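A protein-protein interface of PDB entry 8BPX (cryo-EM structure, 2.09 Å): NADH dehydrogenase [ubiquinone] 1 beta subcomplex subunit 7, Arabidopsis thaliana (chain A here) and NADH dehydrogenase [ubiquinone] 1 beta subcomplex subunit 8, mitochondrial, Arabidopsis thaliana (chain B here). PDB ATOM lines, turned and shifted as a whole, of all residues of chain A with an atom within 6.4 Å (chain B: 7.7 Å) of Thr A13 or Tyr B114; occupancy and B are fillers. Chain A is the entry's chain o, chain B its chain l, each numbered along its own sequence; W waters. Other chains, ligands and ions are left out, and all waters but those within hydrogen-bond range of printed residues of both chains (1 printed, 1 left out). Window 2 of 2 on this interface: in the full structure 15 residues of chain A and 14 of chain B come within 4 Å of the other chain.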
ATOM      1  N   MET A  10     -19.711  24.476  25.469  1.00  0.00           N
ATOM      2  CA  MET A  10     -20.505  23.344  25.926  1.00  0.00           C
ATOM      3  C   MET A  10     -20.001  22.826  27.264  1.00  0.00           C
ATOM      4  O   MET A  10     -18.810  22.554  27.434  1.00  0.00           O
ATOM      5  CB  MET A  10     -20.496  22.226  24.889  1.00  0.00           C
ATOM      6  CG  MET A  10     -21.510  21.149  25.195  1.00  0.00           C
ATOM      7  SD  MET A  10     -23.201  21.649  24.829  1.00  0.00           S
ATOM      8  CE  MET A  10     -24.098  20.277  25.547  1.00  0.00           C
ATOM      9  N   ILE A  11     -20.921  22.676  28.209  1.00  0.00           N
ATOM     10  CA  ILE A  11     -20.612  22.233  29.559  1.00  0.00           C
ATOM     11  C   ILE A  11     -21.090  20.808  29.793  1.00  0.00           C
ATOM     12  O   ILE A  11     -20.343  19.964  30.290  1.00  0.00           O
ATOM     13  CB  ILE A  11     -21.217  23.198  30.602  1.00  0.00           C
ATOM     14  CG1 ILE A  11     -20.468  24.529  30.594  1.00  0.00           C
ATOM     15  CG2 ILE A  11     -21.209  22.575  31.979  1.00  0.00           C
ATOM     16  CD1 ILE A  11     -21.327  25.712  30.985  1.00  0.00           C
ATOM     17  N   ALA A  12     -22.338  20.522  29.441  1.00  0.00           N
ATOM     18  CA  ALA A  12     -22.874  19.184  29.617  1.00  0.00           C
ATOM     19  C   ALA A  12     -22.190  18.227  28.655  1.00  0.00           C
ATOM     20  O   ALA A  12     -22.013  18.541  27.474  1.00  0.00           O
ATOM     21  CB  ALA A  12     -24.386  19.184  29.396  1.00  0.00           C
ATOM     22  N   THR A  13     -21.776  17.076  29.165  1.00  0.00           N
ATOM     23  CA  THR A  13     -21.199  16.048  28.316  1.00  0.00           C
ATOM     24  C   THR A  13     -22.301  15.249  27.628  1.00  0.00           C
ATOM     25  O   THR A  13     -23.488  15.375  27.937  1.00  0.00           O
ATOM     26  CB  THR A  13     -20.302  15.112  29.126  1.00  0.00           C
ATOM     27  OG1 THR A  13     -21.117  14.226  29.904  1.00  0.00           O
ATOM     28  CG2 THR A  13     -19.391  15.906  30.041  1.00  0.00           C
ATOM     29  N   GLN A  14     -21.890  14.422  26.668  1.00  0.00           N
ATOM     30  CA  GLN A  14     -22.841  13.547  25.996  1.00  0.00           C
ATOM     31  C   GLN A  14     -23.437  12.539  26.968  1.00  0.00           C
ATOM     32  O   GLN A  14     -24.642  12.260  26.930  1.00  0.00           O
ATOM     33  CB  GLN A  14     -22.165  12.833  24.832  1.00  0.00           C
ATOM     34  CG  GLN A  14     -22.196  13.604  23.542  1.00  0.00           C
ATOM     35  CD  GLN A  14     -20.985  13.354  22.669  1.00  0.00           C
ATOM     36  OE1 GLN A  14     -19.868  13.216  23.157  1.00  0.00           O
ATOM     37  NE2 GLN A  14     -21.211  13.270  21.365  1.00  0.00           N
ATOM     38  N   GLU A  15     -22.602  11.998  27.856  1.00  0.00           N
ATOM     39  CA  GLU A  15     -23.068  11.014  28.825  1.00  0.00           C
ATOM     40  C   GLU A  15     -24.129  11.603  29.746  1.00  0.00           C
ATOM     41  O   GLU A  15     -25.135  10.950  30.037  1.00  0.00           O
ATOM     42  CB  GLU A  15     -21.875  10.480  29.623  1.00  0.00           C
ATOM     43  CG  GLU A  15     -22.212   9.629  30.849  1.00  0.00           C
ATOM     44  CD  GLU A  15     -22.602  10.453  32.067  1.00  0.00           C
ATOM     45  OE1 GLU A  15     -21.866  11.403  32.404  1.00  0.00           O
ATOM     46  OE2 GLU A  15     -23.649  10.154  32.677  1.00  0.00           O
ATOM     47  N   GLU A  16     -23.914  12.829  30.223  1.00  0.00           N
ATOM     48  CA  GLU A  16     -24.881  13.452  31.119  1.00  0.00           C
ATOM     49  C   GLU A  16     -26.211  13.691  30.418  1.00  0.00           C
ATOM     50  O   GLU A  16     -27.278  13.442  30.992  1.00  0.00           O
ATOM     51  CB  GLU A  16     -24.314  14.762  31.664  1.00  0.00           C
ATOM     52  CG  GLU A  16     -23.179  14.581  32.645  1.00  0.00           C
ATOM     53  CD  GLU A  16     -22.244  15.771  32.675  1.00  0.00           C
ATOM     54  OE1 GLU A  16     -22.685  16.884  32.339  1.00  0.00           O
ATOM     55  OE2 GLU A  16     -21.063  15.590  33.027  1.00  0.00           O
ATOM     56  N   MET A  17     -26.166  14.169  29.174  1.00  0.00           N
ATOM     57  CA  MET A  17     -27.398  14.436  28.442  1.00  0.00           C
ATOM     58  C   MET A  17     -28.155  13.150  28.139  1.00  0.00           C
ATOM     59  O   MET A  17     -29.390  13.133  28.176  1.00  0.00           O
ATOM     60  CB  MET A  17     -27.094  15.209  27.159  1.00  0.00           C
ATOM     61  CG  MET A  17     -26.759  16.671  27.418  1.00  0.00           C
ATOM     62  SD  MET A  17     -26.562  17.657  25.930  1.00  0.00           S
ATOM     63  CE  MET A  17     -25.217  16.801  25.127  1.00  0.00           C
ATOM     64  N   SER A  18     -27.436  12.063  27.837  1.00  0.00           N
ATOM     65  CA  SER A  18     -28.097  10.779  27.615  1.00  0.00           C
ATOM     66  C   SER A  18     -28.687  10.224  28.907  1.00  0.00           C
ATOM     67  O   SER A  18     -29.789   9.664  28.901  1.00  0.00           O
ATOM     68  CB  SER A  18     -27.120   9.775  27.007  1.00  0.00           C
ATOM     69  OG  SER A  18     -26.893  10.041  25.639  1.00  0.00           O
ATOM     70  N   ARG A  27     -30.566  19.481  23.277  1.00  0.00           N
ATOM     71  CA  ARG A  27     -29.145  19.153  23.611  1.00  0.00           C
ATOM     72  C   ARG A  27     -28.233  20.282  23.080  1.00  0.00           C
ATOM     73  O   ARG A  27     -27.383  20.020  22.291  1.00  0.00           O
ATOM     74  CB  ARG A  27     -28.781  17.719  23.208  1.00  0.00           C
ATOM     75  CG  ARG A  27     -29.593  16.624  23.872  1.00  0.00           C
ATOM     76  CD  ARG A  27     -29.051  15.242  23.584  1.00  0.00           C
ATOM     77  NE  ARG A  27     -29.797  14.296  24.383  1.00  0.00           N
ATOM     78  CZ  ARG A  27     -29.582  12.988  24.463  1.00  0.00           C
ATOM     79  NH1 ARG A  27     -28.608  12.416  23.786  1.00  0.00           N
ATOM     80  NH2 ARG A  27     -30.350  12.255  25.238  1.00  0.00           N
ATOM     81  N   ILE A  35     -30.922  20.069  32.772  1.00  0.00           N
ATOM     82  CA  ILE A  35     -30.929  18.882  33.632  1.00  0.00           C
ATOM     83  C   ILE A  35     -31.501  19.172  35.018  1.00  0.00           C
ATOM     84  O   ILE A  35     -32.450  18.478  35.429  1.00  0.00           O
ATOM     85  CB  ILE A  35     -29.519  18.265  33.686  1.00  0.00           C
ATOM     86  CG1 ILE A  35     -29.076  17.807  32.293  1.00  0.00           C
ATOM     87  CG2 ILE A  35     -29.462  17.122  34.677  1.00  0.00           C
ATOM     88  CD1 ILE A  35     -27.653  17.322  32.232  1.00  0.00           C
ATOM     89  N   VAL B 111     -26.902  25.664  15.641  1.00  0.00           N
ATOM     90  CA  VAL B 111     -25.738  24.774  15.432  1.00  0.00           C
ATOM     91  C   VAL B 111     -25.614  24.047  16.731  1.00  0.00           C
ATOM     92  O   VAL B 111     -25.316  24.660  17.727  1.00  0.00           O
ATOM     93  CB  VAL B 111     -24.446  25.470  14.957  1.00  0.00           C
ATOM     94  CG1 VAL B 111     -23.285  24.495  14.926  1.00  0.00           C
ATOM     95  CG2 VAL B 111     -24.624  26.146  13.616  1.00  0.00           C
ATOM     96  N   TYR B 112     -25.868  22.769  16.647  1.00  0.00           N
ATOM     97  CA  TYR B 112     -25.806  21.930  17.833  1.00  0.00           C
ATOM     98  C   TYR B 112     -24.355  21.559  18.067  1.00  0.00           C
ATOM     99  O   TYR B 112     -23.639  21.491  17.114  1.00  0.00           O
ATOM    100  CB  TYR B 112     -26.773  20.743  17.676  1.00  0.00           C
ATOM    101  CG  TYR B 112     -28.195  21.165  17.897  1.00  0.00           C
ATOM    102  CD1 TYR B 112     -28.937  21.745  16.881  1.00  0.00           C
ATOM    103  CD2 TYR B 112     -28.765  21.047  19.146  1.00  0.00           C
ATOM    104  CE1 TYR B 112     -30.243  22.143  17.099  1.00  0.00           C
ATOM    105  CE2 TYR B 112     -30.068  21.433  19.375  1.00  0.00           C
ATOM    106  CZ  TYR B 112     -30.808  21.978  18.345  1.00  0.00           C
ATOM    107  OH  TYR B 112     -32.083  22.366  18.584  1.00  0.00           O
ATOM    108  N   PRO B 113     -23.971  21.234  19.304  1.00  0.00           N
ATOM    109  CA  PRO B 113     -22.625  20.729  19.599  1.00  0.00           C
ATOM    110  C   PRO B 113     -22.413  19.294  19.144  1.00  0.00           C
ATOM    111  O   PRO B 113     -23.339  18.635  18.654  1.00  0.00           O
ATOM    112  CB  PRO B 113     -22.538  20.846  21.126  1.00  0.00           C
ATOM    113  CG  PRO B 113     -23.956  20.707  21.570  1.00  0.00           C
ATOM    114  CD  PRO B 113     -24.769  21.418  20.529  1.00  0.00           C
ATOM    115  N   TYR B 114     -21.180  18.816  19.304  1.00  0.00           N
ATOM    116  CA  TYR B 114     -20.779  17.450  18.980  1.00  0.00           C
ATOM    117  C   TYR B 114     -21.102  17.106  17.527  1.00  0.00           C
ATOM    118  O   TYR B 114     -21.788  16.131  17.221  1.00  0.00           O
ATOM    119  CB  TYR B 114     -21.416  16.457  19.952  1.00  0.00           C
ATOM    120  CG  TYR B 114     -21.059  16.755  21.386  1.00  0.00           C
ATOM    121  CD1 TYR B 114     -19.779  16.518  21.864  1.00  0.00           C
ATOM    122  CD2 TYR B 114     -21.994  17.293  22.259  1.00  0.00           C
ATOM    123  CE1 TYR B 114     -19.440  16.797  23.165  1.00  0.00           C
ATOM    124  CE2 TYR B 114     -21.664  17.574  23.567  1.00  0.00           C
ATOM    125  CZ  TYR B 114     -20.384  17.323  24.013  1.00  0.00           C
ATOM    126  OH  TYR B 114     -20.049  17.597  25.314  1.00  0.00           O
ATOM    127  N   ASP B 115     -20.567  17.939  16.633  1.00  0.00           N
ATOM    128  CA  ASP B 115     -20.723  17.782  15.188  1.00  0.00           C
ATOM    129  C   ASP B 115     -22.204  17.735  14.806  1.00  0.00           C
ATOM    130  O   ASP B 115     -22.656  16.878  14.044  1.00  0.00           O
ATOM    131  CB  ASP B 115     -19.962  16.549  14.691  1.00  0.00           C
ATOM    132  CG  ASP B 115     -20.006  16.395  13.184  1.00  0.00           C
ATOM    133  OD1 ASP B 115     -20.068  15.243  12.706  1.00  0.00           O
ATOM    134  OD2 ASP B 115     -19.985  17.425  12.480  1.00  0.00           O
ATOM    135  N   ASN B 116     -22.966  18.679  15.285  1.00  0.00           N
ATOM    136  CA  ASN B 116     -24.420  18.754  15.021  1.00  0.00           C
ATOM    137  C   ASN B 116     -25.125  17.459  15.500  1.00  0.00           C
ATOM    138  O   ASN B 116     -26.056  17.121  14.878  1.00  0.00           O
ATOM    139  CB  ASN B 116     -24.687  19.351  13.632  1.00  0.00           C
ATOM    140  CG  ASN B 116     -25.264  20.739  13.703  1.00  0.00           C
ATOM    141  OD1 ASN B 116     -26.393  20.925  14.140  1.00  0.00           O
ATOM    142  ND2 ASN B 116     -24.475  21.717  13.301  1.00  0.00           N
ATOM    143  N   LEU B 117     -24.733  16.938  16.687  1.00  0.00           N
ATOM    144  CA  LEU B 117     -25.338  15.724  17.235  1.00  0.00           C
ATOM    145  C   LEU B 117     -25.359  14.597  16.206  1.00  0.00           C
ATOM    146  O   LEU B 117     -26.389  13.974  15.948  1.00  0.00           O
ATOM    147  CB  LEU B 117     -26.746  16.003  17.765  1.00  0.00           C
ATOM    148  CG  LEU B 117     -26.925  17.098  18.816  1.00  0.00           C
ATOM    149  CD1 LEU B 117     -28.393  17.438  18.973  1.00  0.00           C
ATOM    150  CD2 LEU B 117     -26.325  16.663  20.142  1.00  0.00           C
ATOM    151  N   ARG B 118     -24.195  14.336  15.613  1.00  0.00           N
ATOM    152  CA  ARG B 118     -24.110  13.314  14.578  1.00  0.00           C
ATOM    153  C   ARG B 118     -24.359  11.928  15.160  1.00  0.00           C
ATOM    154  O   ARG B 118     -25.161  11.155  14.627  1.00  0.00           O
ATOM    155  CB  ARG B 118     -22.747  13.381  13.887  1.00  0.00           C
ATOM    156  CG  ARG B 118     -22.527  12.306  12.833  1.00  0.00           C
ATOM    157  CD  ARG B 118     -21.068  12.183  12.436  1.00  0.00           C
ATOM    158  NE  ARG B 118     -20.315  11.312  13.328  1.00  0.00           N
ATOM    159  CZ  ARG B 118     -19.476  11.738  14.260  1.00  0.00           C
ATOM    160  NH1 ARG B 118     -19.259  13.029  14.456  1.00  0.00           N
ATOM    161  NH2 ARG B 118     -18.844  10.850  15.020  1.00  0.00           N
ATOM    162  N   VAL B 119     -23.690  11.604  16.268  1.00  0.00           N
ATOM    163  CA  VAL B 119     -23.831  10.281  16.863  1.00  0.00           C
ATOM    164  C   VAL B 119     -25.205  10.114  17.503  1.00  0.00           C
ATOM    165  O   VAL B 119     -25.838   9.062  17.375  1.00  0.00           O
ATOM    166  CB  VAL B 119     -22.693  10.025  17.868  1.00  0.00           C
ATOM    167  CG1 VAL B 119     -22.857   8.667  18.521  1.00  0.00           C
ATOM    168  CG2 VAL B 119     -21.345  10.129  17.171  1.00  0.00           C
ATOM    169  N   GLU B 120     -25.690  11.147  18.198  1.00  0.00           N
ATOM    170  CA  GLU B 120     -26.997  11.071  18.845  1.00  0.00           C
ATOM    171  C   GLU B 120     -28.136  10.938  17.845  1.00  0.00           C
ATOM    172  O   GLU B 120     -29.220  10.484  18.221  1.00  0.00           O
ATOM    173  CB  GLU B 120     -27.232  12.300  19.725  1.00  0.00           C
ATOM    174  CG  GLU B 120     -26.293  12.406  20.915  1.00  0.00           C
ATOM    175  CD  GLU B 120     -24.899  12.846  20.523  1.00  0.00           C
ATOM    176  OE1 GLU B 120     -24.731  13.402  19.422  1.00  0.00           O
ATOM    177  OE2 GLU B 120     -23.965  12.605  21.304  1.00  0.00           O
HETATM  178  O   HOH W   1     -25.828  13.117  24.159  1.00  0.00           O
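O of Ala A12 is in hydrogen-bond range of OH of Tyr B114 (3.1 Å). The side-chain carboxylate (OE2) of Glu B120 is in hydrogen-bond range of the side-chain amide nitrogen (NE2) of Gln A14 (2.8 Å).
Water W1 lies within hydrogen-bond range of NH1 of Arg A27 (2.9 Å), O of Gln A14 (3.1 Å) and OE2 of Glu B120 (3.4 Å).
The side-chain amide oxygen (OD1) of Asn B116 lies within hydrogen-bond range of the backbone NH (N) of Tyr B112 (3.2 Å). The side-chain hydroxyl (OG1) of Thr A13 lies close to the backbone NH (N) of Glu A15 (3.4 Å). The side-chain hydroxyl (OG1) of Thr A13 is in hydrogen-bond range of the backbone NH (N) of Glu A16, 3.1 Å away. The backbone carbonyl oxygen (O) of Gln A14 sits at hydrogen-bond distance from the side-chain hydroxyl (OG) of Ser A18, at 3.4 Å. NH2 of Arg A27 is in hydrogen-bond range of O of Met A17 (3.2 Å). NH1 of Arg A27 sits at hydrogen-bond distance from OG of Ser A18, at 3.5 Å.
Thr A13 touches just one residue of chain B: Tyr B114 (3.6 Å). Of the printed residues of chain B, Gln A14 touches Tyr B114 and Glu B120. Of the printed residues of chain B, Arg A27 touches Tyr B112 (3.6 Å), Pro B113 (3.4 Å) and Glu B120 (3.7 Å). Of the printed residues of chain A, Tyr B112 touches Arg A27. Of the printed residues of chain A, Pro B113 touches Met A10 and Arg A27. Of chain A, only Met A10 (3.8 Å), Ala A12 (3.1 Å), Thr A13 (3.6 Å), Gln A14 (3.5 Å) and Met A17 (3.96 Å) come within 4 Å of Tyr B114. Printed residues of chain A within 4 Å of Glu B120: Gln A14 (2.8 Å) and Arg A27 (3.7 Å). The nearest residue of chain B that does not touch Thr A13 is Glu B120 (7.1 Å). The nearest residue of chain A that does not touch Tyr B114 is Ile A11 (5.5 Å).
Among the printed residues, merely in contact across the chains: Arg A27 with Pro B113 (3.4 Å), Met A10 with Pro B113 (3.5 Å), Gln A14 with Tyr B114 (3.5 Å), Thr A13 with Tyr B114 (3.6 Å), Arg A27 with Tyr B112 (3.6 Å), Arg A27 with Glu B120 (3.7 Å), Met A10 with Tyr B114 (3.8 Å) and Met A17 with Tyr B114 (3.96 Å).
Hydrophobic or aromatic side chains of chain B within 4 Å of the printed part of chain A: Tyr B112, Pro B113 and Tyr B114. Printed residues of chain A that touch a printed residue of chain B: Met A10, Ala A12, Thr A13, Gln A14, Met A17 and Arg A27. Hydrophobic or aromatic side chains of chain A that line the printed part of chain B: Met A10 and Met A17. Among the printed residues, 10 pairs touch across the chains. Among the printed residues, no Asp or Glu carboxylate lies within 4 Å of a Lys or Arg side-chain nitrogen of the other chain.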
